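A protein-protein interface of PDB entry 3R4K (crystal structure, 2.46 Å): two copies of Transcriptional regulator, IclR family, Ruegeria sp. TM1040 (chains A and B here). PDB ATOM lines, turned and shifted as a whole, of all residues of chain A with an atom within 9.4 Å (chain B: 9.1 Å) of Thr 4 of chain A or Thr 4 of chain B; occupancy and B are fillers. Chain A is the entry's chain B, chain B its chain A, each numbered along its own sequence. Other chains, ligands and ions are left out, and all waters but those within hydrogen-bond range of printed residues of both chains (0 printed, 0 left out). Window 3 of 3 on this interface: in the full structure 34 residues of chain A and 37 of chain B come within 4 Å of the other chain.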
ATOM      1  N   GLY A   3      18.452   2.020  19.791  1.00  0.00           N
ATOM      2  CA  GLY A   3      17.438   1.772  20.810  1.00  0.00           C
ATOM      3  C   GLY A   3      16.921   0.341  20.862  1.00  0.00           C
ATOM      4  O   GLY A   3      16.747  -0.298  19.817  1.00  0.00           O
ATOM      5  N   THR A   4      16.637  -0.159  22.084  1.00  0.00           N
ATOM      6  CA  THR A   4      16.148  -1.517  22.354  1.00  0.00           C
ATOM      7  C   THR A   4      14.753  -1.767  21.698  1.00  0.00           C
ATOM      8  O   THR A   4      14.516  -2.885  21.213  1.00  0.00           O
ATOM      9  CB  THR A   4      16.171  -1.824  23.878  1.00  0.00           C
ATOM     10  OG1 THR A   4      15.984  -3.223  24.107  1.00  0.00           O
ATOM     11  CG2 THR A   4      15.154  -1.012  24.692  1.00  0.00           C
ATOM     12  N   VAL A   5      13.861  -0.733  21.652  1.00  0.00           N
ATOM     13  CA  VAL A   5      12.535  -0.851  21.010  1.00  0.00           C
ATOM     14  C   VAL A   5      12.720  -1.080  19.500  1.00  0.00           C
ATOM     15  O   VAL A   5      12.145  -2.030  18.956  1.00  0.00           O
ATOM     16  CB  VAL A   5      11.617   0.381  21.276  1.00  0.00           C
ATOM     17  CG1 VAL A   5      10.270   0.241  20.554  1.00  0.00           C
ATOM     18  CG2 VAL A   5      11.415   0.625  22.769  1.00  0.00           C
ATOM     19  N   SER A   6      13.551  -0.211  18.853  1.00  0.00           N
ATOM     20  CA  SER A   6      13.859  -0.247  17.423  1.00  0.00           C
ATOM     21  C   SER A   6      14.555  -1.557  17.041  1.00  0.00           C
ATOM     22  O   SER A   6      14.266  -2.093  15.970  1.00  0.00           O
ATOM     23  CB  SER A   6      14.711   0.956  17.015  1.00  0.00           C
ATOM     24  OG  SER A   6      16.040   0.890  17.510  1.00  0.00           O
ATOM     25  N   LYS A   7      15.462  -2.088  17.930  1.00  0.00           N
ATOM     26  CA  LYS A   7      16.206  -3.348  17.730  1.00  0.00           C
ATOM     27  C   LYS A   7      15.243  -4.526  17.659  1.00  0.00           C
ATOM     28  O   LYS A   7      15.353  -5.377  16.764  1.00  0.00           O
ATOM     29  CB  LYS A   7      17.209  -3.579  18.875  1.00  0.00           C
ATOM     30  CG  LYS A   7      18.639  -3.248  18.538  1.00  0.00           C
ATOM     31  CD  LYS A   7      19.497  -3.234  19.803  1.00  0.00           C
ATOM     32  CE  LYS A   7      20.190  -4.561  20.090  1.00  0.00           C
ATOM     33  NZ  LYS A   7      21.331  -4.427  21.038  1.00  0.00           N
ATOM     34  N   ALA A   8      14.285  -4.551  18.605  1.00  0.00           N
ATOM     35  CA  ALA A   8      13.271  -5.585  18.699  1.00  0.00           C
ATOM     36  C   ALA A   8      12.386  -5.599  17.457  1.00  0.00           C
ATOM     37  O   ALA A   8      12.132  -6.662  16.890  1.00  0.00           O
ATOM     38  CB  ALA A   8      12.427  -5.364  19.950  1.00  0.00           C
ATOM     39  N   LEU A   9      11.957  -4.422  17.007  1.00  0.00           N
ATOM     40  CA  LEU A   9      11.073  -4.315  15.849  1.00  0.00           C
ATOM     41  C   LEU A   9      11.808  -4.621  14.534  1.00  0.00           C
ATOM     42  O   LEU A   9      11.157  -5.084  13.600  1.00  0.00           O
ATOM     43  CB  LEU A   9      10.363  -2.948  15.816  1.00  0.00           C
ATOM     44  CG  LEU A   9       9.519  -2.649  17.072  1.00  0.00           C
ATOM     45  CD1 LEU A   9       9.088  -1.217  17.143  1.00  0.00           C
ATOM     46  CD2 LEU A   9       8.351  -3.581  17.211  1.00  0.00           C
ATOM     47  N   THR A  10      13.143  -4.452  14.474  1.00  0.00           N
ATOM     48  CA  THR A  10      13.979  -4.830  13.307  1.00  0.00           C
ATOM     49  C   THR A  10      13.941  -6.366  13.104  1.00  0.00           C
ATOM     50  O   THR A  10      13.984  -6.835  11.967  1.00  0.00           O
ATOM     51  CB  THR A  10      15.431  -4.344  13.514  1.00  0.00           C
ATOM     52  OG1 THR A  10      15.412  -2.924  13.632  1.00  0.00           O
ATOM     53  CG2 THR A  10      16.388  -4.779  12.412  1.00  0.00           C
ATOM     54  N   LEU A  11      13.846  -7.131  14.208  1.00  0.00           N
ATOM     55  CA  LEU A  11      13.789  -8.597  14.145  1.00  0.00           C
ATOM     56  C   LEU A  11      12.550  -9.087  13.361  1.00  0.00           C
ATOM     57  O   LEU A  11      12.628 -10.096  12.653  1.00  0.00           O
ATOM     58  CB  LEU A  11      13.821  -9.213  15.568  1.00  0.00           C
ATOM     59  CG  LEU A  11      15.141  -9.090  16.340  1.00  0.00           C
ATOM     60  CD1 LEU A  11      14.971  -9.538  17.753  1.00  0.00           C
ATOM     61  CD2 LEU A  11      16.220  -9.930  15.704  1.00  0.00           C
ATOM     62  N   MET A  33      22.943  -9.917  15.818  1.00  0.00           N
ATOM     63  CA  MET A  33      22.909  -9.767  17.279  1.00  0.00           C
ATOM     64  C   MET A  33      23.264 -11.098  17.938  1.00  0.00           C
ATOM     65  O   MET A  33      23.130 -12.146  17.299  1.00  0.00           O
ATOM     66  CB  MET A  33      21.501  -9.300  17.753  1.00  0.00           C
ATOM     67  CG  MET A  33      20.887  -8.146  16.954  1.00  0.00           C
ATOM     68  SD  MET A  33      19.107  -7.684  17.625  1.00  0.00           S
ATOM     69  CE  MET A  33      18.460  -6.645  16.149  1.00  0.00           C
ATOM     70  N   THR A  37      20.672 -11.814  23.131  1.00  0.00           N
ATOM     71  CA  THR A  37      19.983 -10.553  22.830  1.00  0.00           C
ATOM     72  C   THR A  37      18.703 -10.854  22.077  1.00  0.00           C
ATOM     73  O   THR A  37      17.648 -10.347  22.458  1.00  0.00           O
ATOM     74  CB  THR A  37      20.889  -9.590  22.042  1.00  0.00           C
ATOM     75  OG1 THR A  37      22.047  -9.303  22.824  1.00  0.00           O
ATOM     76  CG2 THR A  37      20.177  -8.279  21.665  1.00  0.00           C
ATOM     77  N   ARG A  40      16.070 -12.535  24.350  1.00  0.00           N
ATOM     78  CA  ARG A  40      15.437 -11.585  25.272  1.00  0.00           C
ATOM     79  C   ARG A  40      14.428 -10.696  24.558  1.00  0.00           C
ATOM     80  O   ARG A  40      13.322 -10.511  25.070  1.00  0.00           O
ATOM     81  CB  ARG A  40      16.484 -10.727  25.983  1.00  0.00           C
ATOM     82  CG  ARG A  40      15.909  -9.681  26.951  1.00  0.00           C
ATOM     83  CD  ARG A  40      16.868  -9.354  28.082  1.00  0.00           C
ATOM     84  NE  ARG A  40      18.164  -8.847  27.619  1.00  0.00           N
ATOM     85  CZ  ARG A  40      19.310  -9.527  27.659  1.00  0.00           C
ATOM     86  NH1 ARG A  40      19.337 -10.778  28.120  1.00  0.00           N
ATOM     87  NH2 ARG A  40      20.433  -8.965  27.237  1.00  0.00           N
ATOM     88  N   LEU A  41      14.806 -10.159  23.380  1.00  0.00           N
ATOM     89  CA  LEU A  41      13.952  -9.290  22.583  1.00  0.00           C
ATOM     90  C   LEU A  41      12.744 -10.052  22.061  1.00  0.00           C
ATOM     91  O   LEU A  41      11.633  -9.525  22.137  1.00  0.00           O
ATOM     92  CB  LEU A  41      14.746  -8.666  21.423  1.00  0.00           C
ATOM     93  CG  LEU A  41      15.851  -7.648  21.806  1.00  0.00           C
ATOM     94  CD1 LEU A  41      16.581  -7.148  20.568  1.00  0.00           C
ATOM     95  CD2 LEU A  41      15.276  -6.442  22.581  1.00  0.00           C
ATOM     96  N   MET A  42      12.942 -11.295  21.564  1.00  0.00           N
ATOM     97  CA  MET A  42      11.839 -12.109  21.045  1.00  0.00           C
ATOM     98  C   MET A  42      10.901 -12.551  22.178  1.00  0.00           C
ATOM     99  O   MET A  42       9.704 -12.680  21.914  1.00  0.00           O
ATOM    100  CB  MET A  42      12.332 -13.325  20.252  1.00  0.00           C
ATOM    101  CG  MET A  42      12.996 -12.957  18.949  1.00  0.00           C
ATOM    102  SD  MET A  42      11.824 -12.092  17.665  1.00  0.00           S
ATOM    103  CE  MET A  42      10.951 -13.634  16.996  1.00  0.00           C
ATOM    104  N   GLU A  44      10.240 -10.734  24.877  1.00  0.00           N
ATOM    105  CA  GLU A  44       9.521  -9.506  25.195  1.00  0.00           C
ATOM    106  C   GLU A  44       8.409  -9.285  24.172  1.00  0.00           C
ATOM    107  O   GLU A  44       7.304  -8.909  24.555  1.00  0.00           O
ATOM    108  CB  GLU A  44      10.490  -8.318  25.275  1.00  0.00           C
ATOM    109  CG  GLU A  44      11.082  -8.163  26.669  1.00  0.00           C
ATOM    110  CD  GLU A  44      11.931  -6.923  26.896  1.00  0.00           C
ATOM    111  OE1 GLU A  44      13.121  -6.928  26.509  1.00  0.00           O
ATOM    112  OE2 GLU A  44      11.417  -5.953  27.507  1.00  0.00           O
ATOM    113  N   LEU A  45       8.672  -9.601  22.890  1.00  0.00           N
ATOM    114  CA  LEU A  45       7.682  -9.511  21.814  1.00  0.00           C
ATOM    115  C   LEU A  45       6.621 -10.598  21.975  1.00  0.00           C
ATOM    116  O   LEU A  45       5.451 -10.357  21.701  1.00  0.00           O
ATOM    117  CB  LEU A  45       8.353  -9.635  20.444  1.00  0.00           C
ATOM    118  CG  LEU A  45       9.176  -8.447  19.973  1.00  0.00           C
ATOM    119  CD1 LEU A  45      10.137  -8.862  18.867  1.00  0.00           C
ATOM    120  CD2 LEU A  45       8.291  -7.319  19.510  1.00  0.00           C
ATOM    121  N   GLU A  47       5.646 -12.005  24.931  1.00  0.00           N
ATOM    122  CA  GLU A  47       4.809 -11.643  26.080  1.00  0.00           C
ATOM    123  C   GLU A  47       3.700 -10.675  25.640  1.00  0.00           C
ATOM    124  O   GLU A  47       2.575 -10.773  26.132  1.00  0.00           O
ATOM    125  CB  GLU A  47       5.657 -11.031  27.212  1.00  0.00           C
ATOM    126  CG  GLU A  47       6.483 -12.032  28.013  1.00  0.00           C
ATOM    127  CD  GLU A  47       7.767 -11.541  28.674  1.00  0.00           C
ATOM    128  OE1 GLU A  47       8.577 -12.402  29.091  1.00  0.00           O
ATOM    129  OE2 GLU A  47       7.943 -10.309  28.821  1.00  0.00           O
ATOM    130  N   MET B   2       8.637  -5.877  32.646  1.00  0.00           N
ATOM    131  CA  MET B   2       8.544  -4.434  32.909  1.00  0.00           C
ATOM    132  C   MET B   2       9.735  -3.639  32.324  1.00  0.00           C
ATOM    133  O   MET B   2       9.984  -2.500  32.724  1.00  0.00           O
ATOM    134  CB  MET B   2       8.374  -4.115  34.411  1.00  0.00           C
ATOM    135  CG  MET B   2       9.320  -4.867  35.320  1.00  0.00           C
ATOM    136  SD  MET B   2       8.505  -6.525  35.943  1.00  0.00           S
ATOM    137  CE  MET B   2       7.543  -5.811  37.537  1.00  0.00           C
ATOM    138  N   GLY B   3      10.413  -4.234  31.352  1.00  0.00           N
ATOM    139  CA  GLY B   3      11.492  -3.608  30.600  1.00  0.00           C
ATOM    140  C   GLY B   3      10.972  -2.567  29.627  1.00  0.00           C
ATOM    141  O   GLY B   3       9.757  -2.448  29.437  1.00  0.00           O
ATOM    142  N   THR B   4      11.893  -1.825  28.983  1.00  0.00           N
ATOM    143  CA  THR B   4      11.588  -0.725  28.055  1.00  0.00           C
ATOM    144  C   THR B   4      10.837  -1.204  26.794  1.00  0.00           C
ATOM    145  O   THR B   4       9.968  -0.465  26.314  1.00  0.00           O
ATOM    146  CB  THR B   4      12.829   0.121  27.702  1.00  0.00           C
ATOM    147  OG1 THR B   4      14.035  -0.558  28.050  1.00  0.00           O
ATOM    148  CG2 THR B   4      12.826   1.430  28.424  1.00  0.00           C
ATOM    149  N   VAL B   5      11.103  -2.441  26.295  1.00  0.00           N
ATOM    150  CA  VAL B   5      10.400  -2.967  25.115  1.00  0.00           C
ATOM    151  C   VAL B   5       8.929  -3.235  25.504  1.00  0.00           C
ATOM    152  O   VAL B   5       8.025  -2.790  24.795  1.00  0.00           O
ATOM    153  CB  VAL B   5      11.101  -4.198  24.486  1.00  0.00           C
ATOM    154  CG1 VAL B   5      10.242  -4.854  23.397  1.00  0.00           C
ATOM    155  CG2 VAL B   5      12.458  -3.819  23.930  1.00  0.00           C
ATOM    156  N   SER B   6       8.714  -3.901  26.663  1.00  0.00           N
ATOM    157  CA  SER B   6       7.412  -4.203  27.260  1.00  0.00           C
ATOM    158  C   SER B   6       6.597  -2.929  27.523  1.00  0.00           C
ATOM    159  O   SER B   6       5.399  -2.908  27.262  1.00  0.00           O
ATOM    160  CB  SER B   6       7.600  -4.956  28.576  1.00  0.00           C
ATOM    161  OG  SER B   6       7.930  -6.323  28.376  1.00  0.00           O
ATOM    162  N   LYS B   7       7.258  -1.873  28.049  1.00  0.00           N
ATOM    163  CA  LYS B   7       6.661  -0.573  28.358  1.00  0.00           C
ATOM    164  C   LYS B   7       6.125   0.095  27.098  1.00  0.00           C
ATOM    165  O   LYS B   7       4.985   0.575  27.095  1.00  0.00           O
ATOM    166  CB  LYS B   7       7.679   0.353  29.030  1.00  0.00           C
ATOM    167  CG  LYS B   7       7.599   0.365  30.547  1.00  0.00           C
ATOM    168  CD  LYS B   7       8.865   0.932  31.200  1.00  0.00           C
ATOM    169  CE  LYS B   7       8.806   2.409  31.429  1.00  0.00           C
ATOM    170  NZ  LYS B   7      10.020   2.914  32.116  1.00  0.00           N
ATOM    171  N   ALA B   8       6.944   0.089  26.019  1.00  0.00           N
ATOM    172  CA  ALA B   8       6.597   0.675  24.730  1.00  0.00           C
ATOM    173  C   ALA B   8       5.392  -0.028  24.120  1.00  0.00           C
ATOM    174  O   ALA B   8       4.463   0.635  23.656  1.00  0.00           O
ATOM    175  CB  ALA B   8       7.786   0.585  23.795  1.00  0.00           C
ATOM    176  N   LEU B   9       5.380  -1.370  24.167  1.00  0.00           N
ATOM    177  CA  LEU B   9       4.305  -2.148  23.580  1.00  0.00           C
ATOM    178  C   LEU B   9       3.002  -2.031  24.374  1.00  0.00           C
ATOM    179  O   LEU B   9       1.940  -2.120  23.764  1.00  0.00           O
ATOM    180  CB  LEU B   9       4.724  -3.612  23.379  1.00  0.00           C
ATOM    181  CG  LEU B   9       5.927  -3.796  22.455  1.00  0.00           C
ATOM    182  CD1 LEU B   9       6.458  -5.205  22.525  1.00  0.00           C
ATOM    183  CD2 LEU B   9       5.637  -3.302  21.004  1.00  0.00           C
ATOM    184  N   THR B  10       3.075  -1.751  25.690  1.00  0.00           N
ATOM    185  CA  THR B  10       1.901  -1.537  26.550  1.00  0.00           C
ATOM    186  C   THR B  10       1.148  -0.280  26.092  1.00  0.00           C
ATOM    187  O   THR B  10      -0.079  -0.259  26.153  1.00  0.00           O
ATOM    188  CB  THR B  10       2.334  -1.431  28.017  1.00  0.00           C
ATOM    189  OG1 THR B  10       2.946  -2.656  28.405  1.00  0.00           O
ATOM    190  CG2 THR B  10       1.192  -1.150  28.952  1.00  0.00           C
ATOM    191  N   LEU B  11       1.887   0.754  25.620  1.00  0.00           N
ATOM    192  CA  LEU B  11       1.304   2.013  25.159  1.00  0.00           C
ATOM    193  C   LEU B  11       0.339   1.784  23.989  1.00  0.00           C
ATOM    194  O   LEU B  11      -0.695   2.456  23.922  1.00  0.00           O
ATOM    195  CB  LEU B  11       2.394   3.040  24.772  1.00  0.00           C
ATOM    196  CG  LEU B  11       3.249   3.611  25.925  1.00  0.00           C
ATOM    197  CD1 LEU B  11       4.415   4.441  25.388  1.00  0.00           C
ATOM    198  CD2 LEU B  11       2.417   4.467  26.858  1.00  0.00           C
ATOM    199  N   MET B  33       3.118   6.378  33.250  1.00  0.00           N
ATOM    200  CA  MET B  33       4.515   6.742  32.987  1.00  0.00           C
ATOM    201  C   MET B  33       4.681   8.264  32.906  1.00  0.00           C
ATOM    202  O   MET B  33       3.697   8.963  32.666  1.00  0.00           O
ATOM    203  CB  MET B  33       4.999   6.109  31.667  1.00  0.00           C
ATOM    204  CG  MET B  33       4.665   4.619  31.529  1.00  0.00           C
ATOM    205  SD  MET B  33       5.267   3.870  29.848  1.00  0.00           S
ATOM    206  CE  MET B  33       4.202   2.368  29.780  1.00  0.00           C
ATOM    207  N   THR B  37       9.044   9.892  29.310  1.00  0.00           N
ATOM    208  CA  THR B  37       9.170   8.467  29.018  1.00  0.00           C
ATOM    209  C   THR B  37       8.271   8.116  27.842  1.00  0.00           C
ATOM    210  O   THR B  37       8.736   7.492  26.880  1.00  0.00           O
ATOM    211  CB  THR B  37       8.842   7.610  30.248  1.00  0.00           C
ATOM    212  OG1 THR B  37       9.745   7.926  31.303  1.00  0.00           O
ATOM    213  CG2 THR B  37       8.915   6.108  29.953  1.00  0.00           C
ATOM    214  N   ARG B  40       9.547   9.569  24.534  1.00  0.00           N
ATOM    215  CA  ARG B  40      10.740   8.837  24.104  1.00  0.00           C
ATOM    216  C   ARG B  40      10.384   7.501  23.446  1.00  0.00           C
ATOM    217  O   ARG B  40      10.949   7.156  22.404  1.00  0.00           O
ATOM    218  CB  ARG B  40      11.650   8.584  25.307  1.00  0.00           C
ATOM    219  CG  ARG B  40      13.095   8.995  25.086  1.00  0.00           C
ATOM    220  CD  ARG B  40      13.965   8.696  26.303  1.00  0.00           C
ATOM    221  NE  ARG B  40      13.725   9.602  27.438  1.00  0.00           N
ATOM    222  CZ  ARG B  40      13.197   9.232  28.604  1.00  0.00           C
ATOM    223  NH1 ARG B  40      12.833   7.968  28.808  1.00  0.00           N
ATOM    224  NH2 ARG B  40      13.034  10.120  29.577  1.00  0.00           N
ATOM    225  N   LEU B  41       9.455   6.764  24.066  1.00  0.00           N
ATOM    226  CA  LEU B  41       8.976   5.464  23.619  1.00  0.00           C
ATOM    227  C   LEU B  41       8.116   5.602  22.360  1.00  0.00           C
ATOM    228  O   LEU B  41       8.253   4.784  21.440  1.00  0.00           O
ATOM    229  CB  LEU B  41       8.173   4.771  24.746  1.00  0.00           C
ATOM    230  CG  LEU B  41       8.949   4.327  25.995  1.00  0.00           C
ATOM    231  CD1 LEU B  41       8.017   3.709  27.025  1.00  0.00           C
ATOM    232  CD2 LEU B  41      10.043   3.335  25.657  1.00  0.00           C
ATOM    233  N   MET B  42       7.240   6.636  22.306  1.00  0.00           N
ATOM    234  CA  MET B  42       6.381   6.856  21.133  1.00  0.00           C
ATOM    235  C   MET B  42       7.211   7.310  19.912  1.00  0.00           C
ATOM    236  O   MET B  42       6.853   6.978  18.782  1.00  0.00           O
ATOM    237  CB  MET B  42       5.250   7.842  21.432  1.00  0.00           C
ATOM    238  CG  MET B  42       4.211   7.290  22.402  1.00  0.00           C
ATOM    239  SD  MET B  42       3.275   5.713  21.803  1.00  0.00           S
ATOM    240  CE  MET B  42       2.067   6.612  20.662  1.00  0.00           C
ATOM    241  N   GLU B  44      10.354   6.245  19.313  1.00  0.00           N
ATOM    242  CA  GLU B  44      10.984   5.004  18.912  1.00  0.00           C
ATOM    243  C   GLU B  44       9.999   4.155  18.106  1.00  0.00           C
ATOM    244  O   GLU B  44      10.403   3.535  17.122  1.00  0.00           O
ATOM    245  CB  GLU B  44      11.495   4.241  20.141  1.00  0.00           C
ATOM    246  CG  GLU B  44      12.939   4.540  20.474  1.00  0.00           C
ATOM    247  CD  GLU B  44      13.541   3.630  21.522  1.00  0.00           C
ATOM    248  OE1 GLU B  44      13.393   3.951  22.724  1.00  0.00           O
ATOM    249  OE2 GLU B  44      14.150   2.597  21.147  1.00  0.00           O
ATOM    250  N   LEU B  45       8.707   4.161  18.488  1.00  0.00           N
ATOM    251  CA  LEU B  45       7.653   3.428  17.773  1.00  0.00           C
ATOM    252  C   LEU B  45       7.367   4.107  16.431  1.00  0.00           C
ATOM    253  O   LEU B  45       7.114   3.426  15.443  1.00  0.00           O
ATOM    254  CB  LEU B  45       6.386   3.319  18.617  1.00  0.00           C
ATOM    255  CG  LEU B  45       6.474   2.359  19.809  1.00  0.00           C
ATOM    256  CD1 LEU B  45       5.408   2.670  20.836  1.00  0.00           C
ATOM    257  CD2 LEU B  45       6.392   0.877  19.368  1.00  0.00           C
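N of Ser 6 of chain B lies within hydrogen-bond range of OE2 of Glu 44 of chain A (3.5 Å).
The backbone NH (N) of Val 5 of chain A sits close to the side-chain carboxylate (OE2) of Glu 44 of chain B, at 3.4 Å.
O of Ser 6 of chain A lies within hydrogen-bond range of OG1 of Thr 10 of chain A (2.7 Å).
O of Gly 3 of chain A is in hydrogen-bond range of OG of Ser 6 of chain A.
O of Ser 6 of chain B lies within hydrogen-bond range of OG1 of Thr 10 of chain B (2.7 Å).
Among the printed residues, merely in contact across the chains: Gly 3 of chain A with Glu 44 of chain B, Glu 44 of chain A with Val 5 of chain B, Thr 4 of chain A with Val 5 of chain B, Thr 4 of chain A with Thr 4 of chain B, Ser 6 of chain A with Glu 44 of chain B, Val 5 of chain A with Ala 8 of chain B, Thr 4 of chain A with Glu 44 of chain B, Glu 44 of chain A with Gly 3 of chain B and Val 5 of chain A with Thr 4 of chain B.
Of the printed residues of chain A, Thr 4 of chain B touches Thr 4 and Val 5.
Of chain A, only Glu 44 comes within 4 Å of Gly 3 of chain B.
Val 5 of chain B touches just these residues of chain A: Thr 4 and Glu 44.
No residue of chain A comes within 4 Å of Lys 7 of chain B.
Of the printed residues of chain A, Glu 44 of chain B touches Gly 3, Thr 4, Val 5 and Ser 6.
Of the printed residues of chain B, Ser 6 of chain A touches Glu 44 (3.7 Å).
Of the printed residues of chain B, Val 5 of chain A touches Thr 4 (3.98 Å), Ala 8 (3.8 Å) and Glu 44 (3.4 Å).
Leu 11 of chain A touches none of the printed residues of chain B.
Printed residues of chain B that touch a printed residue of chain A: Gly 3, Thr 4, Val 5, Ser 6, Ala 8 and Glu 44.
Of the 17 printed residues of chain A, 5 touch a printed residue of chain B.
Among the printed residues, 11 pairs touch across the chains.
Gly 3 of chain A touches Glu 44 of chain B, and with the chains exchanged Glu 44 of chain A touches Gly 3 of chain B.
Thr 4 of chain A touches Val 5 of chain B, and with the chains exchanged Val 5 of chain A touches Thr 4 of chain B.
Val 5 of chain A touches Ala 8 of chain B, but with the chains exchanged Ala 8 of chain A does not touch Val 5 of chain B (4.1 Å).
Val 5 of chain A touches Glu 44 of chain B, and with the chains exchanged Glu 44 of chain A touches Val 5 of chain B.
Positions printed for both chains: 3, 4, 5, 6, 7, 8, 9, 10, 11, 33, 37, 40, 41, 42, 44 and 45.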
